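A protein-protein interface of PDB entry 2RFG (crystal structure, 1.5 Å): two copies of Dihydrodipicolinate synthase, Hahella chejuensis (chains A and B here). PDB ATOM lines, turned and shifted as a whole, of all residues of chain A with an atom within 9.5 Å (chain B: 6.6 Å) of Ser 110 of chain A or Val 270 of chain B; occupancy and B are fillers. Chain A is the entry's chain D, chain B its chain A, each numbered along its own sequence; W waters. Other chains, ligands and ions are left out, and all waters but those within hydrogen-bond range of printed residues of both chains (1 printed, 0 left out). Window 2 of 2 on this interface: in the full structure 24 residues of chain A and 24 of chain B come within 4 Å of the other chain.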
ATOM      1  N   PRO A  81     -10.185 -23.880   6.584  1.00  0.00           N
ATOM      2  CA  PRO A  81     -10.907 -25.102   6.168  1.00  0.00           C
ATOM      3  C   PRO A  81     -12.051 -24.857   5.173  1.00  0.00           C
ATOM      4  O   PRO A  81     -12.380 -25.764   4.404  1.00  0.00           O
ATOM      5  CB  PRO A  81     -11.435 -25.682   7.487  1.00  0.00           C
ATOM      6  CG  PRO A  81     -11.428 -24.528   8.459  1.00  0.00           C
ATOM      7  CD  PRO A  81     -10.257 -23.671   8.045  1.00  0.00           C
ATOM      8  N   ALA A 103      -2.982 -28.263   6.973  1.00  0.00           N
ATOM      9  CA  ALA A 103      -3.795 -27.280   7.696  1.00  0.00           C
ATOM     10  C   ALA A 103      -2.911 -26.416   8.590  1.00  0.00           C
ATOM     11  O   ALA A 103      -1.801 -26.811   8.929  1.00  0.00           O
ATOM     12  CB  ALA A 103      -4.864 -27.990   8.537  1.00  0.00           C
ATOM     13  N   GLY A 104      -3.410 -25.242   8.969  1.00  0.00           N
ATOM     14  CA  GLY A 104      -2.875 -24.535  10.130  1.00  0.00           C
ATOM     15  C   GLY A 104      -1.590 -23.747   9.973  1.00  0.00           C
ATOM     16  O   GLY A 104      -1.103 -23.180  10.957  1.00  0.00           O
ATOM     17  N   ASN A 107      -1.626 -19.259  10.679  1.00  0.00           N
ATOM     18  CA  ASN A 107      -2.529 -19.012  11.819  1.00  0.00           C
ATOM     19  C   ASN A 107      -2.248 -19.851  13.077  1.00  0.00           C
ATOM     20  O   ASN A 107      -2.603 -19.439  14.194  1.00  0.00           O
ATOM     21  CB  ASN A 107      -4.026 -19.002  11.444  1.00  0.00           C
ATOM     22  CG  ASN A 107      -4.462 -20.208  10.627  1.00  0.00           C
ATOM     23  OD1 ASN A 107      -3.726 -21.191  10.462  1.00  0.00           O
ATOM     24  ND2 ASN A 107      -5.688 -20.130  10.111  1.00  0.00           N
ATOM     25  N   ARG A 108      -1.585 -21.000  12.894  1.00  0.00           N
ATOM     26  CA  ARG A 108      -1.021 -21.761  14.024  1.00  0.00           C
ATOM     27  C   ARG A 108      -2.047 -22.164  15.092  1.00  0.00           C
ATOM     28  O   ARG A 108      -1.900 -21.814  16.283  1.00  0.00           O
ATOM     29  CB  ARG A 108       0.117 -20.966  14.684  1.00  0.00           C
ATOM     30  CG  ARG A 108       1.523 -21.446  14.398  1.00  0.00           C
ATOM     31  CD  ARG A 108       2.556 -20.575  15.140  1.00  0.00           C
ATOM     32  NE  ARG A 108       2.022 -19.986  16.376  1.00  0.00           N
ATOM     33  CZ  ARG A 108       2.578 -18.976  17.047  1.00  0.00           C
ATOM     34  NH1 ARG A 108       3.710 -18.419  16.624  1.00  0.00           N
ATOM     35  NH2 ARG A 108       1.998 -18.517  18.147  1.00  0.00           N
ATOM     36  N   PRO A 109      -3.092 -22.912  14.697  1.00  0.00           N
ATOM     37  CA  PRO A 109      -4.121 -23.337  15.642  1.00  0.00           C
ATOM     38  C   PRO A 109      -3.655 -24.444  16.585  1.00  0.00           C
ATOM     39  O   PRO A 109      -2.579 -25.035  16.395  1.00  0.00           O
ATOM     40  CB  PRO A 109      -5.214 -23.876  14.718  1.00  0.00           C
ATOM     41  CG  PRO A 109      -4.455 -24.407  13.544  1.00  0.00           C
ATOM     42  CD  PRO A 109      -3.364 -23.397  13.333  1.00  0.00           C
ATOM     43  N   SER A 110      -4.489 -24.716  17.583  1.00  0.00           N
ATOM     44  CA  SER A 110      -4.310 -25.822  18.524  1.00  0.00           C
ATOM     45  C   SER A 110      -4.560 -27.176  17.860  1.00  0.00           C
ATOM     46  O   SER A 110      -5.044 -27.251  16.727  1.00  0.00           O
ATOM     47  CB  SER A 110      -5.311 -25.652  19.665  1.00  0.00           C
ATOM     48  OG  SER A 110      -6.639 -25.830  19.183  1.00  0.00           O
ATOM     49  N   GLN A 111      -4.265 -28.256  18.585  1.00  0.00           N
ATOM     50  CA  GLN A 111      -4.587 -29.598  18.096  1.00  0.00           C
ATOM     51  C   GLN A 111      -6.079 -29.769  17.842  1.00  0.00           C
ATOM     52  O   GLN A 111      -6.474 -30.407  16.865  1.00  0.00           O
ATOM     53  CB  GLN A 111      -4.091 -30.675  19.067  1.00  0.00           C
ATOM     54  CG  GLN A 111      -2.579 -30.678  19.282  1.00  0.00           C
ATOM     55  CD  GLN A 111      -1.806 -31.012  18.019  1.00  0.00           C
ATOM     56  OE1 GLN A 111      -1.892 -32.128  17.508  1.00  0.00           O
ATOM     57  NE2 GLN A 111      -1.038 -30.049  17.512  1.00  0.00           N
ATOM     58  N   GLU A 112      -6.906 -29.182  18.710  1.00  0.00           N
ATOM     59  CA  GLU A 112      -8.346 -29.219  18.531  1.00  0.00           C
ATOM     60  C   GLU A 112      -8.755 -28.484  17.247  1.00  0.00           C
ATOM     61  O   GLU A 112      -9.626 -28.953  16.508  1.00  0.00           O
ATOM     62  CB  GLU A 112      -9.049 -28.638  19.757  1.00  0.00           C
ATOM     63  CG  GLU A 112     -10.571 -28.538  19.629  1.00  0.00           C
ATOM     64  CD  GLU A 112     -11.286 -29.882  19.573  1.00  0.00           C
ATOM     65  OE1 GLU A 112     -10.714 -30.918  19.999  1.00  0.00           O
ATOM     66  OE2 GLU A 112     -12.452 -29.898  19.116  1.00  0.00           O
ATOM     67  N   GLY A 113      -8.132 -27.336  16.984  1.00  0.00           N
ATOM     68  CA  GLY A 113      -8.402 -26.600  15.748  1.00  0.00           C
ATOM     69  C   GLY A 113      -8.009 -27.378  14.501  1.00  0.00           C
ATOM     70  O   GLY A 113      -8.761 -27.410  13.523  1.00  0.00           O
ATOM     71  N   LEU A 114      -6.841 -28.022  14.534  1.00  0.00           N
ATOM     72  CA  LEU A 114      -6.428 -28.898  13.431  1.00  0.00           C
ATOM     73  C   LEU A 114      -7.438 -30.029  13.216  1.00  0.00           C
ATOM     74  O   LEU A 114      -7.862 -30.283  12.081  1.00  0.00           O
ATOM     75  CB  LEU A 114      -5.027 -29.475  13.685  1.00  0.00           C
ATOM     76  CG  LEU A 114      -3.885 -28.459  13.707  1.00  0.00           C
ATOM     77  CD1 LEU A 114      -2.593 -29.067  14.267  1.00  0.00           C
ATOM     78  CD2 LEU A 114      -3.636 -27.882  12.313  1.00  0.00           C
ATOM     79  N   TYR A 115      -7.834 -30.691  14.303  1.00  0.00           N
ATOM     80  CA  TYR A 115      -8.834 -31.746  14.218  1.00  0.00           C
ATOM     81  C   TYR A 115     -10.126 -31.247  13.557  1.00  0.00           C
ATOM     82  O   TYR A 115     -10.641 -31.888  12.629  1.00  0.00           O
ATOM     83  CB  TYR A 115      -9.128 -32.366  15.594  1.00  0.00           C
ATOM     84  CG  TYR A 115     -10.211 -33.412  15.504  1.00  0.00           C
ATOM     85  CD1 TYR A 115      -9.931 -34.697  15.033  1.00  0.00           C
ATOM     86  CD2 TYR A 115     -11.523 -33.105  15.849  1.00  0.00           C
ATOM     87  CE1 TYR A 115     -10.934 -35.653  14.913  1.00  0.00           C
ATOM     88  CE2 TYR A 115     -12.537 -34.056  15.734  1.00  0.00           C
ATOM     89  CZ  TYR A 115     -12.230 -35.327  15.266  1.00  0.00           C
ATOM     90  OH  TYR A 115     -13.220 -36.283  15.149  1.00  0.00           O
ATOM     91  N   GLN A 116     -10.639 -30.101  14.012  1.00  0.00           N
ATOM     92  CA  GLN A 116     -11.883 -29.569  13.447  1.00  0.00           C
ATOM     93  C   GLN A 116     -11.750 -29.196  11.973  1.00  0.00           C
ATOM     94  O   GLN A 116     -12.694 -29.356  11.203  1.00  0.00           O
ATOM     95  CB  GLN A 116     -12.410 -28.392  14.270  1.00  0.00           C
ATOM     96  CG  GLN A 116     -12.789 -28.758  15.708  1.00  0.00           C
ATOM     97  CD  GLN A 116     -13.943 -29.730  15.802  1.00  0.00           C
ATOM     98  OE1 GLN A 116     -14.801 -29.779  14.924  1.00  0.00           O
ATOM     99  NE2 GLN A 116     -13.973 -30.508  16.877  1.00  0.00           N
ATOM    100  N   HIS A 117     -10.579 -28.693  11.587  1.00  0.00           N
ATOM    101  CA  HIS A 117     -10.299 -28.412  10.177  1.00  0.00           C
ATOM    102  C   HIS A 117     -10.463 -29.684   9.344  1.00  0.00           C
ATOM    103  O   HIS A 117     -11.241 -29.710   8.389  1.00  0.00           O
ATOM    104  CB  HIS A 117      -8.891 -27.829  10.035  1.00  0.00           C
ATOM    105  CG  HIS A 117      -8.448 -27.605   8.618  1.00  0.00           C
ATOM    106  ND1 HIS A 117      -8.006 -26.379   8.162  1.00  0.00           N
ATOM    107  CD2 HIS A 117      -8.338 -28.461   7.569  1.00  0.00           C
ATOM    108  CE1 HIS A 117      -7.656 -26.487   6.891  1.00  0.00           C
ATOM    109  NE2 HIS A 117      -7.850 -27.739   6.507  1.00  0.00           N
ATOM    110  N   PHE A 118      -9.747 -30.747   9.725  1.00  0.00           N
ATOM    111  CA  PHE A 118      -9.799 -31.991   8.969  1.00  0.00           C
ATOM    112  C   PHE A 118     -11.186 -32.620   8.997  1.00  0.00           C
ATOM    113  O   PHE A 118     -11.636 -33.160   7.984  1.00  0.00           O
ATOM    114  CB  PHE A 118      -8.723 -32.976   9.443  1.00  0.00           C
ATOM    115  CG  PHE A 118      -7.327 -32.542   9.102  1.00  0.00           C
ATOM    116  CD1 PHE A 118      -6.931 -32.415   7.772  1.00  0.00           C
ATOM    117  CD2 PHE A 118      -6.411 -32.234  10.107  1.00  0.00           C
ATOM    118  CE1 PHE A 118      -5.634 -31.988   7.448  1.00  0.00           C
ATOM    119  CE2 PHE A 118      -5.115 -31.822   9.790  1.00  0.00           C
ATOM    120  CZ  PHE A 118      -4.729 -31.695   8.463  1.00  0.00           C
ATOM    121  N   VAL A 140       2.932 -25.777  12.831  1.00  0.00           N
ATOM    122  CA  VAL A 140       2.055 -26.725  13.530  1.00  0.00           C
ATOM    123  C   VAL A 140       2.437 -28.165  13.216  1.00  0.00           C
ATOM    124  O   VAL A 140       2.921 -28.487  12.120  1.00  0.00           O
ATOM    125  CB  VAL A 140       0.553 -26.516  13.213  1.00  0.00           C
ATOM    126  CG1 VAL A 140       0.084 -25.206  13.765  1.00  0.00           C
ATOM    127  CG2 VAL A 140       0.278 -26.620  11.720  1.00  0.00           C
ATOM    128  N   ASP A 141       2.214 -29.013  14.206  1.00  0.00           N
ATOM    129  CA  ASP A 141       2.567 -30.419  14.129  1.00  0.00           C
ATOM    130  C   ASP A 141       1.352 -31.186  14.607  1.00  0.00           C
ATOM    131  O   ASP A 141       0.904 -31.003  15.741  1.00  0.00           O
ATOM    132  CB  ASP A 141       3.746 -30.667  15.066  1.00  0.00           C
ATOM    133  CG  ASP A 141       4.292 -32.082  14.996  1.00  0.00           C
ATOM    134  OD1 ASP A 141       3.676 -32.965  14.354  1.00  0.00           O
ATOM    135  OD2 ASP A 141       5.364 -32.295  15.611  1.00  0.00           O
ATOM    136  N   ILE A 142       0.807 -32.022  13.736  1.00  0.00           N
ATOM    137  CA  ILE A 142      -0.246 -32.952  14.125  1.00  0.00           C
ATOM    138  C   ILE A 142       0.404 -34.043  14.982  1.00  0.00           C
ATOM    139  O   ILE A 142       1.118 -34.923  14.474  1.00  0.00           O
ATOM    140  CB  ILE A 142      -0.944 -33.574  12.910  1.00  0.00           C
ATOM    141  CG1 ILE A 142      -1.406 -32.475  11.944  1.00  0.00           C
ATOM    142  CG2 ILE A 142      -2.128 -34.438  13.365  1.00  0.00           C
ATOM    143  CD1 ILE A 142      -1.712 -32.960  10.569  1.00  0.00           C
ATOM    144  N   LYS A 143       0.164 -33.972  16.287  1.00  0.00           N
ATOM    145  CA  LYS A 143       0.802 -34.880  17.230  1.00  0.00           C
ATOM    146  C   LYS A 143       0.201 -36.279  17.129  1.00  0.00           C
ATOM    147  O   LYS A 143      -0.923 -36.433  16.653  1.00  0.00           O
ATOM    148  CB  LYS A 143       0.670 -34.343  18.656  1.00  0.00           C
ATOM    149  CG  LYS A 143       1.285 -32.969  18.872  1.00  0.00           C
ATOM    150  CD  LYS A 143       2.773 -32.949  18.611  1.00  0.00           C
ATOM    151  CE  LYS A 143       3.334 -31.569  18.893  1.00  0.00           C
ATOM    152  NZ  LYS A 143       4.756 -31.498  18.488  1.00  0.00           N
ATOM    153  N   THR A 146      -3.377 -36.778  18.170  1.00  0.00           N
ATOM    154  CA  THR A 146      -4.294 -36.131  17.237  1.00  0.00           C
ATOM    155  C   THR A 146      -4.430 -36.946  15.962  1.00  0.00           C
ATOM    156  O   THR A 146      -5.524 -37.085  15.429  1.00  0.00           O
ATOM    157  CB  THR A 146      -3.825 -34.711  16.901  1.00  0.00           C
ATOM    158  OG1 THR A 146      -3.535 -34.029  18.125  1.00  0.00           O
ATOM    159  CG2 THR A 146      -4.895 -33.943  16.103  1.00  0.00           C
ATOM    160  N   ARG A 149      -6.736 -39.671  16.712  1.00  0.00           N
ATOM    161  CA  ARG A 149      -8.092 -39.149  16.745  1.00  0.00           C
ATOM    162  C   ARG A 149      -8.640 -38.981  15.318  1.00  0.00           C
ATOM    163  O   ARG A 149      -9.782 -39.347  15.033  1.00  0.00           O
ATOM    164  CB  ARG A 149      -8.107 -37.827  17.507  1.00  0.00           C
ATOM    165  CG  ARG A 149      -9.470 -37.349  17.878  1.00  0.00           C
ATOM    166  CD  ARG A 149      -9.360 -36.021  18.586  1.00  0.00           C
ATOM    167  NE  ARG A 149     -10.679 -35.448  18.787  1.00  0.00           N
ATOM    168  CZ  ARG A 149     -10.903 -34.192  19.143  1.00  0.00           C
ATOM    169  NH1 ARG A 149      -9.886 -33.355  19.339  1.00  0.00           N
ATOM    170  NH2 ARG A 149     -12.150 -33.781  19.300  1.00  0.00           N
ATOM    171  N   GLU B 245      -4.173 -19.924  24.965  1.00  0.00           N
ATOM    172  CA  GLU B 245      -4.666 -20.689  23.818  1.00  0.00           C
ATOM    173  C   GLU B 245      -4.392 -19.863  22.550  1.00  0.00           C
ATOM    174  O   GLU B 245      -4.111 -18.663  22.648  1.00  0.00           O
ATOM    175  CB  GLU B 245      -6.161 -20.950  23.988  1.00  0.00           C
ATOM    176  CG  GLU B 245      -6.485 -21.660  25.298  1.00  0.00           C
ATOM    177  CD  GLU B 245      -7.906 -22.197  25.371  1.00  0.00           C
ATOM    178  OE1 GLU B 245      -8.424 -22.697  24.349  1.00  0.00           O
ATOM    179  OE2 GLU B 245      -8.506 -22.152  26.465  1.00  0.00           O
ATOM    180  N   PRO B 246      -4.406 -20.495  21.362  1.00  0.00           N
ATOM    181  CA  PRO B 246      -4.049 -19.720  20.163  1.00  0.00           C
ATOM    182  C   PRO B 246      -4.892 -18.464  19.903  1.00  0.00           C
ATOM    183  O   PRO B 246      -6.120 -18.508  19.744  1.00  0.00           O
ATOM    184  CB  PRO B 246      -4.175 -20.743  19.031  1.00  0.00           C
ATOM    185  CG  PRO B 246      -3.876 -22.037  19.721  1.00  0.00           C
ATOM    186  CD  PRO B 246      -4.605 -21.922  21.030  1.00  0.00           C
ATOM    187  N   ALA B 249      -8.349 -16.159  19.923  1.00  0.00           N
ATOM    188  CA  ALA B 249      -9.458 -16.652  20.768  1.00  0.00           C
ATOM    189  C   ALA B 249      -9.578 -15.834  22.064  1.00  0.00           C
ATOM    190  O   ALA B 249     -10.675 -15.438  22.464  1.00  0.00           O
ATOM    191  CB  ALA B 249      -9.286 -18.136  21.069  1.00  0.00           C
ATOM    192  N   CYS B 265     -14.783 -16.864  16.971  1.00  0.00           N
ATOM    193  CA  CYS B 265     -13.748 -16.811  15.934  1.00  0.00           C
ATOM    194  C   CYS B 265     -14.024 -17.890  14.892  1.00  0.00           C
ATOM    195  O   CYS B 265     -14.817 -18.807  15.135  1.00  0.00           O
ATOM    196  CB  CYS B 265     -12.361 -17.017  16.534  1.00  0.00           C
ATOM    197  SG  CYS B 265     -11.871 -15.752  17.728  1.00  0.00           S
ATOM    198  N   ARG B 266     -13.386 -17.782  13.730  1.00  0.00           N
ATOM    199  CA  ARG B 266     -13.556 -18.797  12.684  1.00  0.00           C
ATOM    200  C   ARG B 266     -12.543 -19.933  12.845  1.00  0.00           C
ATOM    201  O   ARG B 266     -11.372 -19.704  13.172  1.00  0.00           O
ATOM    202  CB  ARG B 266     -13.417 -18.183  11.283  1.00  0.00           C
ATOM    203  CG  ARG B 266     -14.565 -17.298  10.850  1.00  0.00           C
ATOM    204  CD  ARG B 266     -14.382 -16.781   9.435  1.00  0.00           C
ATOM    205  NE  ARG B 266     -15.548 -15.966   9.058  1.00  0.00           N
ATOM    206  CZ  ARG B 266     -15.652 -15.295   7.915  1.00  0.00           C
ATOM    207  NH1 ARG B 266     -14.673 -15.330   7.017  1.00  0.00           N
ATOM    208  NH2 ARG B 266     -16.744 -14.577   7.671  1.00  0.00           N
ATOM    209  N   LEU B 267     -12.985 -21.160  12.587  1.00  0.00           N
ATOM    210  CA  LEU B 267     -12.052 -22.290  12.555  1.00  0.00           C
ATOM    211  C   LEU B 267     -10.879 -21.951  11.620  1.00  0.00           C
ATOM    212  O   LEU B 267     -11.070 -21.343  10.571  1.00  0.00           O
ATOM    213  CB  LEU B 267     -12.765 -23.549  12.061  1.00  0.00           C
ATOM    214  CG  LEU B 267     -13.739 -24.181  13.052  1.00  0.00           C
ATOM    215  CD1 LEU B 267     -14.424 -25.364  12.391  1.00  0.00           C
ATOM    216  CD2 LEU B 267     -13.052 -24.642  14.336  1.00  0.00           C
ATOM    217  N   PRO B 268      -9.649 -22.361  11.977  1.00  0.00           N
ATOM    218  CA  PRO B 268      -9.278 -23.301  13.044  1.00  0.00           C
ATOM    219  C   PRO B 268      -9.057 -22.688  14.438  1.00  0.00           C
ATOM    220  O   PRO B 268      -8.560 -23.371  15.341  1.00  0.00           O
ATOM    221  CB  PRO B 268      -7.974 -23.890  12.500  1.00  0.00           C
ATOM    222  CG  PRO B 268      -7.325 -22.705  11.825  1.00  0.00           C
ATOM    223  CD  PRO B 268      -8.464 -21.906  11.217  1.00  0.00           C
ATOM    224  N   ILE B 269      -9.430 -21.421  14.625  1.00  0.00           N
ATOM    225  CA  ILE B 269      -9.445 -20.851  15.973  1.00  0.00           C
ATOM    226  C   ILE B 269     -10.682 -21.427  16.650  1.00  0.00           C
ATOM    227  O   ILE B 269     -11.735 -21.504  16.026  1.00  0.00           O
ATOM    228  CB  ILE B 269      -9.465 -19.303  15.939  1.00  0.00           C
ATOM    229  CG1 ILE B 269      -8.342 -18.750  15.037  1.00  0.00           C
ATOM    230  CG2 ILE B 269      -9.413 -18.731  17.363  1.00  0.00           C
ATOM    231  CD1 ILE B 269      -6.915 -19.177  15.436  1.00  0.00           C
ATOM    232  N   VAL B 270     -10.537 -21.890  17.888  1.00  0.00           N
ATOM    233  CA  VAL B 270     -11.609 -22.634  18.568  1.00  0.00           C
ATOM    234  C   VAL B 270     -12.018 -21.956  19.887  1.00  0.00           C
ATOM    235  O   VAL B 270     -11.278 -21.128  20.420  1.00  0.00           O
ATOM    236  CB  VAL B 270     -11.222 -24.125  18.809  1.00  0.00           C
ATOM    237  CG1 VAL B 270     -11.045 -24.851  17.483  1.00  0.00           C
ATOM    238  CG2 VAL B 270      -9.979 -24.242  19.684  1.00  0.00           C
ATOM    239  N   PRO B 271     -13.216 -22.296  20.406  1.00  0.00           N
ATOM    240  CA  PRO B 271     -13.630 -21.705  21.683  1.00  0.00           C
ATOM    241  C   PRO B 271     -12.658 -22.003  22.824  1.00  0.00           C
ATOM    242  O   PRO B 271     -12.056 -23.088  22.885  1.00  0.00           O
ATOM    243  CB  PRO B 271     -14.985 -22.370  21.950  1.00  0.00           C
ATOM    244  CG  PRO B 271     -15.493 -22.720  20.586  1.00  0.00           C
ATOM    245  CD  PRO B 271     -14.269 -23.164  19.836  1.00  0.00           C
ATOM    246  N   LEU B 272     -12.498 -21.023  23.713  1.00  0.00           N
ATOM    247  CA  LEU B 272     -11.651 -21.172  24.889  1.00  0.00           C
ATOM    248  C   LEU B 272     -12.193 -22.199  25.864  1.00  0.00           C
ATOM    249  O   LEU B 272     -13.405 -22.443  25.922  1.00  0.00           O
ATOM    250  CB  LEU B 272     -11.566 -19.845  25.633  1.00  0.00           C
ATOM    251  CG  LEU B 272     -10.849 -18.688  24.941  1.00  0.00           C
ATOM    252  CD1 LEU B 272     -10.957 -17.467  25.838  1.00  0.00           C
ATOM    253  CD2 LEU B 272      -9.384 -19.009  24.648  1.00  0.00           C
ATOM    254  N   SER B 273     -11.294 -22.768  26.661  1.00  0.00           N
ATOM    255  CA  SER B 273     -11.726 -23.598  27.785  1.00  0.00           C
ATOM    256  C   SER B 273     -12.368 -22.720  28.862  1.00  0.00           C
ATOM    257  O   SER B 273     -12.152 -21.501  28.896  1.00  0.00           O
ATOM    258  CB  SER B 273     -10.537 -24.353  28.369  1.00  0.00           C
ATOM    259  OG  SER B 273      -9.693 -23.467  29.086  1.00  0.00           O
HETATM  260  O   HOH W   1      -6.878 -23.027  17.574  1.00  0.00           O
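The side-chain amide oxygen (OD1) of Asn 107 of chain A lies close to the backbone carbonyl oxygen (O) of Gly 104 of chain A (3.3 Å).
OG of Ser 110 of chain A lies close to N of Glu 112 of chain A, at 3.4 Å.
The backbone NH (N) of Gly 113 of chain A sits at hydrogen-bond distance from the side-chain hydroxyl (OG) of Ser 110 of chain A, 3.1 Å away.
The side-chain carboxylate (OE2) of Glu 112 of chain A sits at hydrogen-bond distance from the side-chain amide nitrogen (NE2) of Gln 116 of chain A (2.8 Å).
Hydrophobic or aromatic side chains of chain A that line the printed part of chain B: Pro 81 and Pro 109.
Among the printed residues, merely in contact across the chains: Pro 81 of chain A with Leu 267 of chain B (3.5 Å), Asn 107 of chain A with Pro 268 of chain B (3.5 Å), Arg 108 of chain A with Pro 246 of chain B (3.7 Å), Pro 109 of chain A with Pro 246 of chain B (3.96 Å), Pro 109 of chain A with Pro 268 of chain B (3.4 Å), Ser 110 of chain A with Pro 246 of chain B (3.5 Å), Ser 110 of chain A with Val 270 of chain B (3.7 Å), Gly 113 of chain A with Pro 268 of chain B (3.3 Å), Gly 113 of chain A with Val 270 of chain B (3.6 Å) and Gln 116 of chain A with Leu 267 of chain B (3.8 Å).
No position is printed for both chains.
Of the 10 pairs that touch across the chains among the printed residues, none has its exchanged pair printed and touching as well.
Ser 110 of chain A touches just these residues of chain B: Pro 246 and Val 270.
Of chain A, only Ser 110 and Gly 113 come within 4 Å of Val 270 of chain B.
No residue of chain A comes within 4 Å of Ile 269 of chain B.
No residue of chain A comes within 4 Å of Pro 271 of chain B.
Printed residues of chain B within 4 Å of Pro 109 of chain A: Pro 246 and Pro 268.
Printed residues of chain B within 4 Å of Pro 81 of chain A: Leu 267.
Printed residues of chain B within 4 Å of Gly 113 of chain A: Pro 268 (3.3 Å) and Val 270 (3.6 Å).
Of the printed residues of chain A, Leu 267 of chain B touches Pro 81 and Gln 116.
Printed residues of chain B within 4 Å of Arg 108 of chain A: Pro 246.
Ser 273 of chain B touches none of the printed residues of chain A.
Leu 272 of chain B touches none of the printed residues of chain A.
The nearest residue of chain B that does not touch Ser 110 of chain A is Pro 268 of chain B (4.8 Å).
Water W1 bridges O of Pro 268 of chain B (2.8 Å) and N of Ser 110 of chain A (2.9 Å).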
